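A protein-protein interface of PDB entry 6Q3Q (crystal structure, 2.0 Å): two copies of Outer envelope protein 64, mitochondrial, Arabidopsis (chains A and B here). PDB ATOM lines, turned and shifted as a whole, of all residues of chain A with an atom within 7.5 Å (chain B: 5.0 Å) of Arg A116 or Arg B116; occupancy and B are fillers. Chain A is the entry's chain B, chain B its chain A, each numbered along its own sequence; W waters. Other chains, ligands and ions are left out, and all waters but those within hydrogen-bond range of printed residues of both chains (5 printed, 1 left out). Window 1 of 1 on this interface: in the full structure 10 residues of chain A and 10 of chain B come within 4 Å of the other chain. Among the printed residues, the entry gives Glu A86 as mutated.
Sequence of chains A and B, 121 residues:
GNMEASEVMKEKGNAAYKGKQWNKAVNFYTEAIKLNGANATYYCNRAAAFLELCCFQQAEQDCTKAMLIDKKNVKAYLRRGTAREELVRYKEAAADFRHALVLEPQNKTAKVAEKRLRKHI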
ATOM      1  N   LEU A  51     -30.183  18.272  10.677  1.00  0.00           N
ATOM      2  CA  LEU A  51     -29.017  18.854  11.301  1.00  0.00           C
ATOM      3  C   LEU A  51     -29.351  20.106  12.099  1.00  0.00           C
ATOM      4  O   LEU A  51     -28.882  20.261  13.251  1.00  0.00           O
ATOM      5  CB  LEU A  51     -27.948  19.213  10.254  1.00  0.00           C
ATOM      6  CG  LEU A  51     -27.209  18.060   9.593  1.00  0.00           C
ATOM      7  CD1 LEU A  51     -26.249  18.663   8.596  1.00  0.00           C
ATOM      8  CD2 LEU A  51     -26.457  17.215  10.599  1.00  0.00           C
ATOM      9  N   GLU A  52     -30.169  20.986  11.526  1.00  0.00           N
ATOM     10  CA  GLU A  52     -30.494  22.241  12.209  1.00  0.00           C
ATOM     11  C   GLU A  52     -31.375  22.021  13.432  1.00  0.00           C
ATOM     12  O   GLU A  52     -31.390  22.845  14.332  1.00  0.00           O
ATOM     13  CB  GLU A  52     -31.114  23.262  11.251  1.00  0.00           C
ATOM     14  CG  GLU A  52     -30.287  23.545   9.989  1.00  0.00           C
ATOM     15  CD  GLU A  52     -28.812  23.895  10.261  1.00  0.00           C
ATOM     16  OE1 GLU A  52     -28.553  24.677  11.191  1.00  0.00           O
ATOM     17  OE2 GLU A  52     -27.922  23.374   9.546  1.00  0.00           O
ATOM     18  N   PHE A  56     -29.322  14.388  15.074  1.00  0.00           N
ATOM     19  CA  PHE A  56     -28.110  13.892  14.401  1.00  0.00           C
ATOM     20  C   PHE A  56     -28.170  12.449  13.943  1.00  0.00           C
ATOM     21  O   PHE A  56     -27.663  12.126  12.877  1.00  0.00           O
ATOM     22  CB  PHE A  56     -26.863  14.220  15.216  1.00  0.00           C
ATOM     23  CG  PHE A  56     -26.707  15.672  15.460  1.00  0.00           C
ATOM     24  CD1 PHE A  56     -26.570  16.539  14.393  1.00  0.00           C
ATOM     25  CD2 PHE A  56     -26.704  16.181  16.736  1.00  0.00           C
ATOM     26  CE1 PHE A  56     -26.421  17.906  14.614  1.00  0.00           C
ATOM     27  CE2 PHE A  56     -26.624  17.535  16.941  1.00  0.00           C
ATOM     28  CZ  PHE A  56     -26.455  18.389  15.887  1.00  0.00           C
ATOM     29  N   GLY A  81     -20.708  13.724   8.052  1.00  0.00           N
ATOM     30  CA  GLY A  81     -19.548  14.100   8.854  1.00  0.00           C
ATOM     31  C   GLY A  81     -19.913  15.091   9.948  1.00  0.00           C
ATOM     32  O   GLY A  81     -19.455  14.959  11.078  1.00  0.00           O
ATOM     33  N   THR A  82     -20.766  16.061   9.617  1.00  0.00           N
ATOM     34  CA  THR A  82     -21.275  17.027  10.590  1.00  0.00           C
ATOM     35  C   THR A  82     -22.035  16.329  11.724  1.00  0.00           C
ATOM     36  O   THR A  82     -21.808  16.617  12.908  1.00  0.00           O
ATOM     37  CB  THR A  82     -22.165  18.083   9.883  1.00  0.00           C
ATOM     38  OG1 THR A  82     -21.388  18.740   8.888  1.00  0.00           O
ATOM     39  CG2 THR A  82     -22.708  19.112  10.851  1.00  0.00           C
ATOM     40  N   GLU A  85     -19.544  14.231  13.868  1.00  0.00           N
ATOM     41  CA  GLU A  85     -18.784  15.122  14.753  1.00  0.00           C
ATOM     42  C   GLU A  85     -19.590  15.533  15.997  1.00  0.00           C
ATOM     43  O   GLU A  85     -19.068  15.509  17.102  1.00  0.00           O
ATOM     44  CB  GLU A  85     -18.257  16.355  13.995  1.00  0.00           C
ATOM     45  CG  GLU A  85     -17.381  17.236  14.878  1.00  0.00           C
ATOM     46  CD  GLU A  85     -16.694  18.358  14.163  1.00  0.00           C
ATOM     47  OE1 GLU A  85     -16.023  19.180  14.849  1.00  0.00           O
ATOM     48  OE2 GLU A  85     -16.774  18.424  12.926  1.00  0.00           O
ATOM     49  N   GLU A  86     -20.870  15.865  15.816  1.00  0.00           N
ATOM     50  CA  GLU A  86     -21.776  16.179  16.940  1.00  0.00           C
ATOM     51  C   GLU A  86     -21.928  14.995  17.874  1.00  0.00           C
ATOM     52  O   GLU A  86     -22.015  15.165  19.100  1.00  0.00           O
ATOM     53  CB  GLU A  86     -23.144  16.643  16.425  1.00  0.00           C
ATOM     54  CG  GLU A  86     -23.100  18.073  15.901  1.00  0.00           C
ATOM     55  CD  GLU A  86     -23.363  19.151  16.972  1.00  0.00           C
ATOM     56  OE1 GLU A  86     -23.534  18.835  18.178  1.00  0.00           O
ATOM     57  OE2 GLU A  86     -23.434  20.354  16.576  1.00  0.00           O
ATOM     58  N   TYR A  90     -15.439  10.742  15.917  1.00  0.00           N
ATOM     59  CA  TYR A  90     -14.513  11.633  15.238  1.00  0.00           C
ATOM     60  C   TYR A  90     -13.812  11.009  14.068  1.00  0.00           C
ATOM     61  O   TYR A  90     -13.589  11.678  13.061  1.00  0.00           O
ATOM     62  CB  TYR A  90     -13.481  12.152  16.241  1.00  0.00           C
ATOM     63  CG  TYR A  90     -14.042  12.998  17.367  1.00  0.00           C
ATOM     64  CD1 TYR A  90     -14.705  14.190  17.102  1.00  0.00           C
ATOM     65  CD2 TYR A  90     -13.862  12.635  18.690  1.00  0.00           C
ATOM     66  CE1 TYR A  90     -15.183  14.995  18.108  1.00  0.00           C
ATOM     67  CE2 TYR A  90     -14.337  13.437  19.728  1.00  0.00           C
ATOM     68  CZ  TYR A  90     -14.966  14.632  19.434  1.00  0.00           C
ATOM     69  OH  TYR A  90     -15.424  15.436  20.450  1.00  0.00           O
ATOM     70  N   PHE A  97     -15.605  13.626   5.869  1.00  0.00           N
ATOM     71  CA  PHE A  97     -15.065  14.877   5.324  1.00  0.00           C
ATOM     72  C   PHE A  97     -13.923  14.624   4.316  1.00  0.00           C
ATOM     73  O   PHE A  97     -13.765  15.354   3.323  1.00  0.00           O
ATOM     74  CB  PHE A  97     -14.612  15.805   6.448  1.00  0.00           C
ATOM     75  CG  PHE A  97     -15.758  16.449   7.198  1.00  0.00           C
ATOM     76  CD1 PHE A  97     -16.644  17.312   6.532  1.00  0.00           C
ATOM     77  CD2 PHE A  97     -15.929  16.231   8.556  1.00  0.00           C
ATOM     78  CE1 PHE A  97     -17.690  17.914   7.215  1.00  0.00           C
ATOM     79  CE2 PHE A  97     -16.987  16.831   9.232  1.00  0.00           C
ATOM     80  CZ  PHE A  97     -17.841  17.676   8.563  1.00  0.00           C
ATOM     81  N   THR A 109     -15.469  23.833   3.605  1.00  0.00           N
ATOM     82  CA  THR A 109     -16.032  23.307   4.833  1.00  0.00           C
ATOM     83  C   THR A 109     -15.284  22.054   5.265  1.00  0.00           C
ATOM     84  O   THR A 109     -14.903  21.933   6.438  1.00  0.00           O
ATOM     85  CB  THR A 109     -17.548  23.048   4.673  1.00  0.00           C
ATOM     86  OG1 THR A 109     -18.194  24.297   4.389  1.00  0.00           O
ATOM     87  CG2 THR A 109     -18.130  22.424   5.943  1.00  0.00           C
ATOM     88  N   ALA A 110     -15.067  21.149   4.315  1.00  0.00           N
ATOM     89  CA  ALA A 110     -14.406  19.906   4.568  1.00  0.00           C
ATOM     90  C   ALA A 110     -12.921  20.117   4.922  1.00  0.00           C
ATOM     91  O   ALA A 110     -12.409  19.411   5.799  1.00  0.00           O
ATOM     92  CB  ALA A 110     -14.537  18.986   3.384  1.00  0.00           C
ATOM     93  N   LYS A 111     -12.248  21.072   4.265  1.00  0.00           N
ATOM     94  CA  LYS A 111     -10.836  21.380   4.581  1.00  0.00           C
ATOM     95  C   LYS A 111     -10.712  21.887   5.996  1.00  0.00           C
ATOM     96  O   LYS A 111      -9.835  21.460   6.757  1.00  0.00           O
ATOM     97  CB  LYS A 111     -10.263  22.431   3.632  1.00  0.00           C
ATOM     98  CG  LYS A 111      -9.978  21.921   2.237  1.00  0.00           C
ATOM     99  CD  LYS A 111      -9.279  22.974   1.404  1.00  0.00           C
ATOM    100  CE  LYS A 111      -9.178  22.499  -0.027  1.00  0.00           C
ATOM    101  NZ  LYS A 111      -8.430  23.449  -0.896  1.00  0.00           N
ATOM    102  N   VAL A 112     -11.610  22.796   6.353  1.00  0.00           N
ATOM    103  CA  VAL A 112     -11.658  23.327   7.701  1.00  0.00           C
ATOM    104  C   VAL A 112     -11.921  22.207   8.711  1.00  0.00           C
ATOM    105  O   VAL A 112     -11.220  22.108   9.721  1.00  0.00           O
ATOM    106  CB  VAL A 112     -12.653  24.494   7.800  1.00  0.00           C
ATOM    107  CG1 VAL A 112     -12.849  24.903   9.246  1.00  0.00           C
ATOM    108  CG2 VAL A 112     -12.142  25.685   6.982  1.00  0.00           C
ATOM    109  N   ALA A 113     -12.880  21.330   8.400  1.00  0.00           N
ATOM    110  CA  ALA A 113     -13.230  20.205   9.298  1.00  0.00           C
ATOM    111  C   ALA A 113     -12.045  19.303   9.577  1.00  0.00           C
ATOM    112  O   ALA A 113     -11.834  18.895  10.720  1.00  0.00           O
ATOM    113  CB  ALA A 113     -14.380  19.385   8.724  1.00  0.00           C
ATOM    114  N   GLU A 114     -11.302  18.962   8.526  1.00  0.00           N
ATOM    115  CA  GLU A 114     -10.163  18.060   8.703  1.00  0.00           C
ATOM    116  C   GLU A 114      -9.107  18.625   9.615  1.00  0.00           C
ATOM    117  O   GLU A 114      -8.576  17.880  10.413  1.00  0.00           O
ATOM    118  CB  GLU A 114      -9.555  17.602   7.388  1.00  0.00           C
ATOM    119  CG  GLU A 114     -10.488  16.677   6.607  1.00  0.00           C
ATOM    120  CD  GLU A 114     -10.785  15.308   7.268  1.00  0.00           C
ATOM    121  OE1 GLU A 114     -10.396  14.989   8.395  1.00  0.00           O
ATOM    122  OE2 GLU A 114     -11.485  14.537   6.639  1.00  0.00           O
ATOM    123  N   LYS A 115      -8.854  19.924   9.530  1.00  0.00           N
ATOM    124  CA  LYS A 115      -7.911  20.560  10.445  1.00  0.00           C
ATOM    125  C   LYS A 115      -8.397  20.500  11.853  1.00  0.00           C
ATOM    126  O   LYS A 115      -7.618  20.193  12.773  1.00  0.00           O
ATOM    127  CB  LYS A 115      -7.612  22.000  10.025  1.00  0.00           C
ATOM    128  CG  LYS A 115      -6.846  22.017   8.702  1.00  0.00           C
ATOM    129  CD  LYS A 115      -6.568  23.408   8.210  1.00  0.00           C
ATOM    130  CE  LYS A 115      -5.752  23.327   6.923  1.00  0.00           C
ATOM    131  NZ  LYS A 115      -5.766  24.628   6.222  1.00  0.00           N
ATOM    132  N   ARG A 116      -9.700  20.753  12.043  1.00  0.00           N
ATOM    133  CA  ARG A 116     -10.290  20.767  13.388  1.00  0.00           C
ATOM    134  C   ARG A 116     -10.282  19.381  14.011  1.00  0.00           C
ATOM    135  O   ARG A 116     -10.103  19.251  15.229  1.00  0.00           O
ATOM    136  CB  ARG A 116     -11.729  21.352  13.333  1.00  0.00           C
ATOM    137  CG  ARG A 116     -12.465  21.365  14.650  1.00  0.00           C
ATOM    138  CD  ARG A 116     -13.809  22.057  14.536  1.00  0.00           C
ATOM    139  NE  ARG A 116     -14.722  21.324  13.665  1.00  0.00           N
ATOM    140  CZ  ARG A 116     -15.016  21.617  12.398  1.00  0.00           C
ATOM    141  NH1 ARG A 116     -14.515  22.683  11.769  1.00  0.00           N
ATOM    142  NH2 ARG A 116     -15.865  20.823  11.738  1.00  0.00           N
ATOM    143  N   LEU A 117     -10.498  18.351  13.185  1.00  0.00           N
ATOM    144  CA  LEU A 117     -10.643  17.003  13.707  1.00  0.00           C
ATOM    145  C   LEU A 117      -9.305  16.334  14.021  1.00  0.00           C
ATOM    146  O   LEU A 117      -9.315  15.323  14.708  1.00  0.00           O
ATOM    147  CB  LEU A 117     -11.452  16.129  12.731  1.00  0.00           C
ATOM    148  CG  LEU A 117     -12.957  16.495  12.701  1.00  0.00           C
ATOM    149  CD1 LEU A 117     -13.636  15.905  11.475  1.00  0.00           C
ATOM    150  CD2 LEU A 117     -13.640  16.025  13.981  1.00  0.00           C
ATOM    151  N   ARG A 118      -8.186  16.883  13.550  1.00  0.00           N
ATOM    152  CA  ARG A 118      -6.864  16.247  13.754  1.00  0.00           C
ATOM    153  C   ARG A 118      -6.624  15.896  15.213  1.00  0.00           C
ATOM    154  O   ARG A 118      -6.172  14.796  15.516  1.00  0.00           O
ATOM    155  CB  ARG A 118      -5.712  17.121  13.220  1.00  0.00           C
ATOM    156  CG  ARG A 118      -5.499  17.042  11.722  1.00  0.00           C
ATOM    157  CD  ARG A 118      -4.190  17.679  11.262  1.00  0.00           C
ATOM    158  NE  ARG A 118      -4.303  19.097  10.889  1.00  0.00           N
ATOM    159  CZ  ARG A 118      -3.361  19.769  10.224  1.00  0.00           C
ATOM    160  NH1 ARG A 118      -2.240  19.151   9.869  1.00  0.00           N
ATOM    161  NH2 ARG A 118      -3.532  21.053   9.928  1.00  0.00           N
ATOM    162  N   LYS A 119      -6.976  16.818  16.114  1.00  0.00           N
ATOM    163  CA  LYS A 119      -6.768  16.614  17.554  1.00  0.00           C
ATOM    164  C   LYS A 119      -7.537  15.495  18.179  1.00  0.00           C
ATOM    165  O   LYS A 119      -7.211  15.080  19.275  1.00  0.00           O
ATOM    166  CB  LYS A 119      -7.081  17.889  18.326  1.00  0.00           C
ATOM    167  CG  LYS A 119      -8.566  18.288  18.341  1.00  0.00           C
ATOM    168  CD  LYS A 119      -8.829  19.601  19.084  1.00  0.00           C
ATOM    169  CE  LYS A 119      -8.327  20.827  18.336  1.00  0.00           C
ATOM    170  NZ  LYS A 119      -9.168  21.132  17.149  1.00  0.00           N
ATOM    171  N   HIS A 120      -8.577  15.014  17.494  1.00  0.00           N
ATOM    172  CA  HIS A 120      -9.411  13.960  18.033  1.00  0.00           C
ATOM    173  C   HIS A 120      -9.209  12.566  17.404  1.00  0.00           C
ATOM    174  O   HIS A 120      -9.849  11.638  17.838  1.00  0.00           O
ATOM    175  CB  HIS A 120     -10.864  14.293  17.777  1.00  0.00           C
ATOM    176  CG  HIS A 120     -11.351  15.454  18.541  1.00  0.00           C
ATOM    177  ND1 HIS A 120     -11.439  15.466  19.907  1.00  0.00           N
ATOM    178  CD2 HIS A 120     -11.825  16.639  18.120  1.00  0.00           C
ATOM    179  CE1 HIS A 120     -11.921  16.623  20.312  1.00  0.00           C
ATOM    180  NE2 HIS A 120     -12.164  17.357  19.247  1.00  0.00           N
ATOM    181  N   ILE A 121      -8.460  12.476  16.321  1.00  0.00           N
ATOM    182  CA  ILE A 121      -8.334  11.216  15.599  1.00  0.00           C
ATOM    183  C   ILE A 121      -6.922  10.685  15.737  1.00  0.00           C
ATOM    184  O   ILE A 121      -6.669   9.615  15.200  1.00  0.00           O
ATOM    185  CB  ILE A 121      -8.727  11.343  14.112  1.00  0.00           C
ATOM    186  CG1 ILE A 121      -7.818  12.273  13.327  1.00  0.00           C
ATOM    187  CG2 ILE A 121     -10.170  11.863  14.014  1.00  0.00           C
ATOM    188  CD1 ILE A 121      -8.174  12.344  11.850  1.00  0.00           C
ATOM    189  OXT ILE A 121      -6.020  11.295  16.334  1.00  0.00           O
ATOM    190  N   GLU B  85     -16.322  26.201  21.788  1.00  0.00           N
ATOM    191  CA  GLU B  85     -17.174  25.228  21.094  1.00  0.00           C
ATOM    192  C   GLU B  85     -16.999  23.803  21.666  1.00  0.00           C
ATOM    193  O   GLU B  85     -17.970  23.103  21.917  1.00  0.00           O
ATOM    194  CB  GLU B  85     -16.938  25.268  19.589  1.00  0.00           C
ATOM    195  CG  GLU B  85     -17.812  24.279  18.809  1.00  0.00           C
ATOM    196  CD  GLU B  85     -17.700  24.435  17.308  1.00  0.00           C
ATOM    197  OE1 GLU B  85     -18.372  23.669  16.581  1.00  0.00           O
ATOM    198  OE2 GLU B  85     -16.958  25.312  16.840  1.00  0.00           O
ATOM    199  N   PHE B  97     -15.853  34.004  17.475  1.00  0.00           N
ATOM    200  CA  PHE B  97     -15.687  33.936  16.030  1.00  0.00           C
ATOM    201  C   PHE B  97     -16.210  35.222  15.334  1.00  0.00           C
ATOM    202  O   PHE B  97     -15.661  35.661  14.338  1.00  0.00           O
ATOM    203  CB  PHE B  97     -16.353  32.683  15.458  1.00  0.00           C
ATOM    204  CG  PHE B  97     -15.615  31.386  15.765  1.00  0.00           C
ATOM    205  CD1 PHE B  97     -14.345  31.178  15.268  1.00  0.00           C
ATOM    206  CD2 PHE B  97     -16.208  30.375  16.509  1.00  0.00           C
ATOM    207  CE1 PHE B  97     -13.657  30.009  15.502  1.00  0.00           C
ATOM    208  CE2 PHE B  97     -15.527  29.188  16.756  1.00  0.00           C
ATOM    209  CZ  PHE B  97     -14.243  29.013  16.232  1.00  0.00           C
ATOM    210  N   VAL B 112     -17.045  29.717   8.460  1.00  0.00           N
ATOM    211  CA  VAL B 112     -17.471  28.336   8.555  1.00  0.00           C
ATOM    212  C   VAL B 112     -18.034  28.032   9.949  1.00  0.00           C
ATOM    213  O   VAL B 112     -19.122  27.449  10.057  1.00  0.00           O
ATOM    214  CB  VAL B 112     -16.368  27.378   8.117  1.00  0.00           C
ATOM    215  CG1 VAL B 112     -16.732  25.925   8.431  1.00  0.00           C
ATOM    216  CG2 VAL B 112     -16.119  27.542   6.605  1.00  0.00           C
ATOM    217  N   ALA B 113     -17.351  28.497  10.997  1.00  0.00           N
ATOM    218  CA  ALA B 113     -17.784  28.261  12.378  1.00  0.00           C
ATOM    219  C   ALA B 113     -19.162  28.831  12.631  1.00  0.00           C
ATOM    220  O   ALA B 113     -19.994  28.187  13.276  1.00  0.00           O
ATOM    221  CB  ALA B 113     -16.795  28.877  13.394  1.00  0.00           C
ATOM    222  N   GLU B 114     -19.390  30.063  12.176  1.00  0.00           N
ATOM    223  CA  GLU B 114     -20.665  30.710  12.432  1.00  0.00           C
ATOM    224  C   GLU B 114     -21.812  29.951  11.806  1.00  0.00           C
ATOM    225  O   GLU B 114     -22.860  29.856  12.417  1.00  0.00           O
ATOM    226  CB  GLU B 114     -20.692  32.181  12.025  1.00  0.00           C
ATOM    227  CG  GLU B 114     -19.743  33.075  12.825  1.00  0.00           C
ATOM    228  CD  GLU B 114     -20.067  33.288  14.305  1.00  0.00           C
ATOM    229  OE1 GLU B 114     -21.009  32.663  14.797  1.00  0.00           O
ATOM    230  OE2 GLU B 114     -19.383  34.114  15.001  1.00  0.00           O
ATOM    231  N   LYS B 115     -21.622  29.396  10.616  1.00  0.00           N
ATOM    232  CA  LYS B 115     -22.667  28.581   9.985  1.00  0.00           C
ATOM    233  C   LYS B 115     -22.943  27.336  10.794  1.00  0.00           C
ATOM    234  O   LYS B 115     -24.091  26.973  10.993  1.00  0.00           O
ATOM    235  CB  LYS B 115     -22.319  28.238   8.547  1.00  0.00           C
ATOM    236  CG  LYS B 115     -22.332  29.490   7.683  1.00  0.00           C
ATOM    237  CD  LYS B 115     -21.936  29.175   6.257  1.00  0.00           C
ATOM    238  CE  LYS B 115     -21.987  30.420   5.387  1.00  0.00           C
ATOM    239  NZ  LYS B 115     -21.364  30.060   4.089  1.00  0.00           N
ATOM    240  N   ARG B 116     -21.879  26.704  11.284  1.00  0.00           N
ATOM    241  CA  ARG B 116     -22.003  25.483  12.081  1.00  0.00           C
ATOM    242  C   ARG B 116     -22.694  25.734  13.419  1.00  0.00           C
ATOM    243  O   ARG B 116     -23.460  24.882  13.900  1.00  0.00           O
ATOM    244  CB  ARG B 116     -20.619  24.837  12.291  1.00  0.00           C
ATOM    245  CG  ARG B 116     -20.633  23.552  13.086  1.00  0.00           C
ATOM    246  CD  ARG B 116     -19.249  22.911  13.140  1.00  0.00           C
ATOM    247  NE  ARG B 116     -18.272  23.761  13.827  1.00  0.00           N
ATOM    248  CZ  ARG B 116     -17.356  24.533  13.251  1.00  0.00           C
ATOM    249  NH1 ARG B 116     -17.201  24.591  11.919  1.00  0.00           N
ATOM    250  NH2 ARG B 116     -16.542  25.253  14.041  1.00  0.00           N
ATOM    251  N   LEU B 117     -22.439  26.898  14.017  1.00  0.00           N
ATOM    252  CA  LEU B 117     -22.943  27.182  15.348  1.00  0.00           C
ATOM    253  C   LEU B 117     -24.407  27.649  15.346  1.00  0.00           C
ATOM    254  O   LEU B 117     -25.006  27.716  16.410  1.00  0.00           O
ATOM    255  CB  LEU B 117     -22.064  28.246  16.040  1.00  0.00           C
ATOM    256  CG  LEU B 117     -20.680  27.742  16.454  1.00  0.00           C
ATOM    257  CD1 LEU B 117     -19.734  28.901  16.753  1.00  0.00           C
ATOM    258  CD2 LEU B 117     -20.754  26.782  17.626  1.00  0.00           C
ATOM    259  N   ARG B 118     -24.969  28.003  14.176  1.00  0.00           N
ATOM    260  CA  ARG B 118     -26.336  28.542  14.115  1.00  0.00           C
ATOM    261  C   ARG B 118     -27.335  27.641  14.851  1.00  0.00           C
ATOM    262  O   ARG B 118     -28.183  28.122  15.574  1.00  0.00           O
ATOM    263  CB  ARG B 118     -26.789  28.741  12.651  1.00  0.00           C
ATOM    264  CG  ARG B 118     -26.287  30.031  11.996  1.00  0.00           C
ATOM    265  CD  ARG B 118     -26.676  30.052  10.512  1.00  0.00           C
ATOM    266  NE  ARG B 118     -26.165  31.199   9.717  1.00  0.00           N
ATOM    267  CZ  ARG B 118     -25.858  31.179   8.406  1.00  0.00           C
ATOM    268  NH1 ARG B 118     -25.410  32.292   7.824  1.00  0.00           N
ATOM    269  NH2 ARG B 118     -25.968  30.071   7.655  1.00  0.00           N
ATOM    270  N   LYS B 119     -27.189  26.325  14.677  1.00  0.00           N
ATOM    271  CA  LYS B 119     -28.088  25.352  15.287  1.00  0.00           C
ATOM    272  C   LYS B 119     -28.064  25.287  16.790  1.00  0.00           C
ATOM    273  O   LYS B 119     -28.937  24.659  17.385  1.00  0.00           O
ATOM    274  CB  LYS B 119     -27.824  23.964  14.741  1.00  0.00           C
ATOM    275  CG  LYS B 119     -26.463  23.360  15.146  1.00  0.00           C
ATOM    276  CD  LYS B 119     -26.242  21.979  14.535  1.00  0.00           C
ATOM    277  CE  LYS B 119     -25.978  22.005  13.025  1.00  0.00           C
ATOM    278  NZ  LYS B 119     -24.622  22.574  12.713  1.00  0.00           N
ATOM    279  N   HIS B 120     -27.055  25.890  17.409  1.00  0.00           N
ATOM    280  CA  HIS B 120     -26.942  25.886  18.858  1.00  0.00           C
ATOM    281  C   HIS B 120     -27.208  27.205  19.539  1.00  0.00           C
ATOM    282  O   HIS B 120     -27.460  27.187  20.740  1.00  0.00           O
ATOM    283  CB  HIS B 120     -25.523  25.467  19.278  1.00  0.00           C
ATOM    284  CG  HIS B 120     -25.201  24.065  18.932  1.00  0.00           C
ATOM    285  ND1 HIS B 120     -25.875  22.997  19.482  1.00  0.00           N
ATOM    286  CD2 HIS B 120     -24.308  23.555  18.070  1.00  0.00           C
ATOM    287  CE1 HIS B 120     -25.392  21.883  18.972  1.00  0.00           C
ATOM    288  NE2 HIS B 120     -24.425  22.197  18.132  1.00  0.00           N
HETATM  289  O   HOH W   1     -22.475  23.048  15.990  1.00  0.00           O
HETATM  290  O   HOH W   2     -30.060  26.531  12.746  1.00  0.00           O
HETATM  291  O   HOH W   3     -17.112  20.957  16.424  1.00  0.00           O
HETATM  292  O   HOH W   4     -22.911  20.895  14.121  1.00  0.00           O
HETATM  293  O   HOH W   5     -20.599  22.216  17.290  1.00  0.00           O
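Among the printed residues, no Asp or Glu carboxylate lies within 4 Å of a Lys or Arg side-chain nitrogen of the other chain.
Of the printed residues of chain B, Leu A51 touches Lys B119 (3.4 Å). Printed residues of chain B within 4 Å of Glu A52: Lys B119. Printed residues of chain B within 4 Å of Glu A86: Lys B119 and His B120. Ala A113 touches none of the printed residues of chain B. Arg A116 touches just one residue of chain B: Arg B116. Arg B116 touches one residue of chain A. Of the printed residues of chain A, His B120 touches Glu A86. The nearest printed residue of chain B that does not touch Arg A116 is Glu B85 (5.1 Å). The nearest printed residue of chain A that does not touch His B120 is Phe A56 (4.8 Å).
OE2 of Glu A86 is in hydrogen-bond range of NE2 of His B120, at 2.6 Å. NH1 of Arg B116 sits close to NH1 of Arg A116 (3.3 Å).
Among the printed residues, merely in contact across the chains: Leu A51 with Lys B119 (3.4 Å), Glu A52 with Lys B119 (3.7 Å), Phe A56 with Lys B119 (3.8 Å) and Glu A86 with Lys B119 (3.8 Å).
Water W4 lies within hydrogen-bond range of the side-chain carboxylate (OE2) of Glu A86 (2.6 Å) and the side-chain amino group (NZ) of Lys B119 (2.8 Å). Water W3 bridges OE1 of Glu A85 (2.6 Å) and OE1 of Glu B85 (3.0 Å). Water W5 lies within hydrogen-bond range of the side-chain carboxylate (OE1) of Glu B85 (2.8 Å) and the side-chain carboxylate (OE2) of Glu A86 (3.5 Å). Water W2 lies within hydrogen-bond range of the side-chain carboxylate of Glu A52 and the backbone NH of Lys B119. Water W1 lies within hydrogen-bond range of the side-chain carboxylate of Glu A86, the backbone carbonyl oxygen of Arg B116 and a ring nitrogen (NE2) of His B120.
Arg B116 touches its own counterpart, Arg A116. 11 positions are printed for both chains.
NZ of Lys A119 lies within hydrogen-bond range of O of Arg A116, at 2.8 Å. NE of Arg B116 is in salt-bridge range of OE1 of Glu B85 (2.8 Å). The side-chain amino group (NZ) of Lys B119 lies within hydrogen-bond range of the backbone carbonyl oxygen (O) of Arg B116, 2.8 Å away. OE1 of Glu A85 lies within salt-bridge range of NE of Arg A116.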
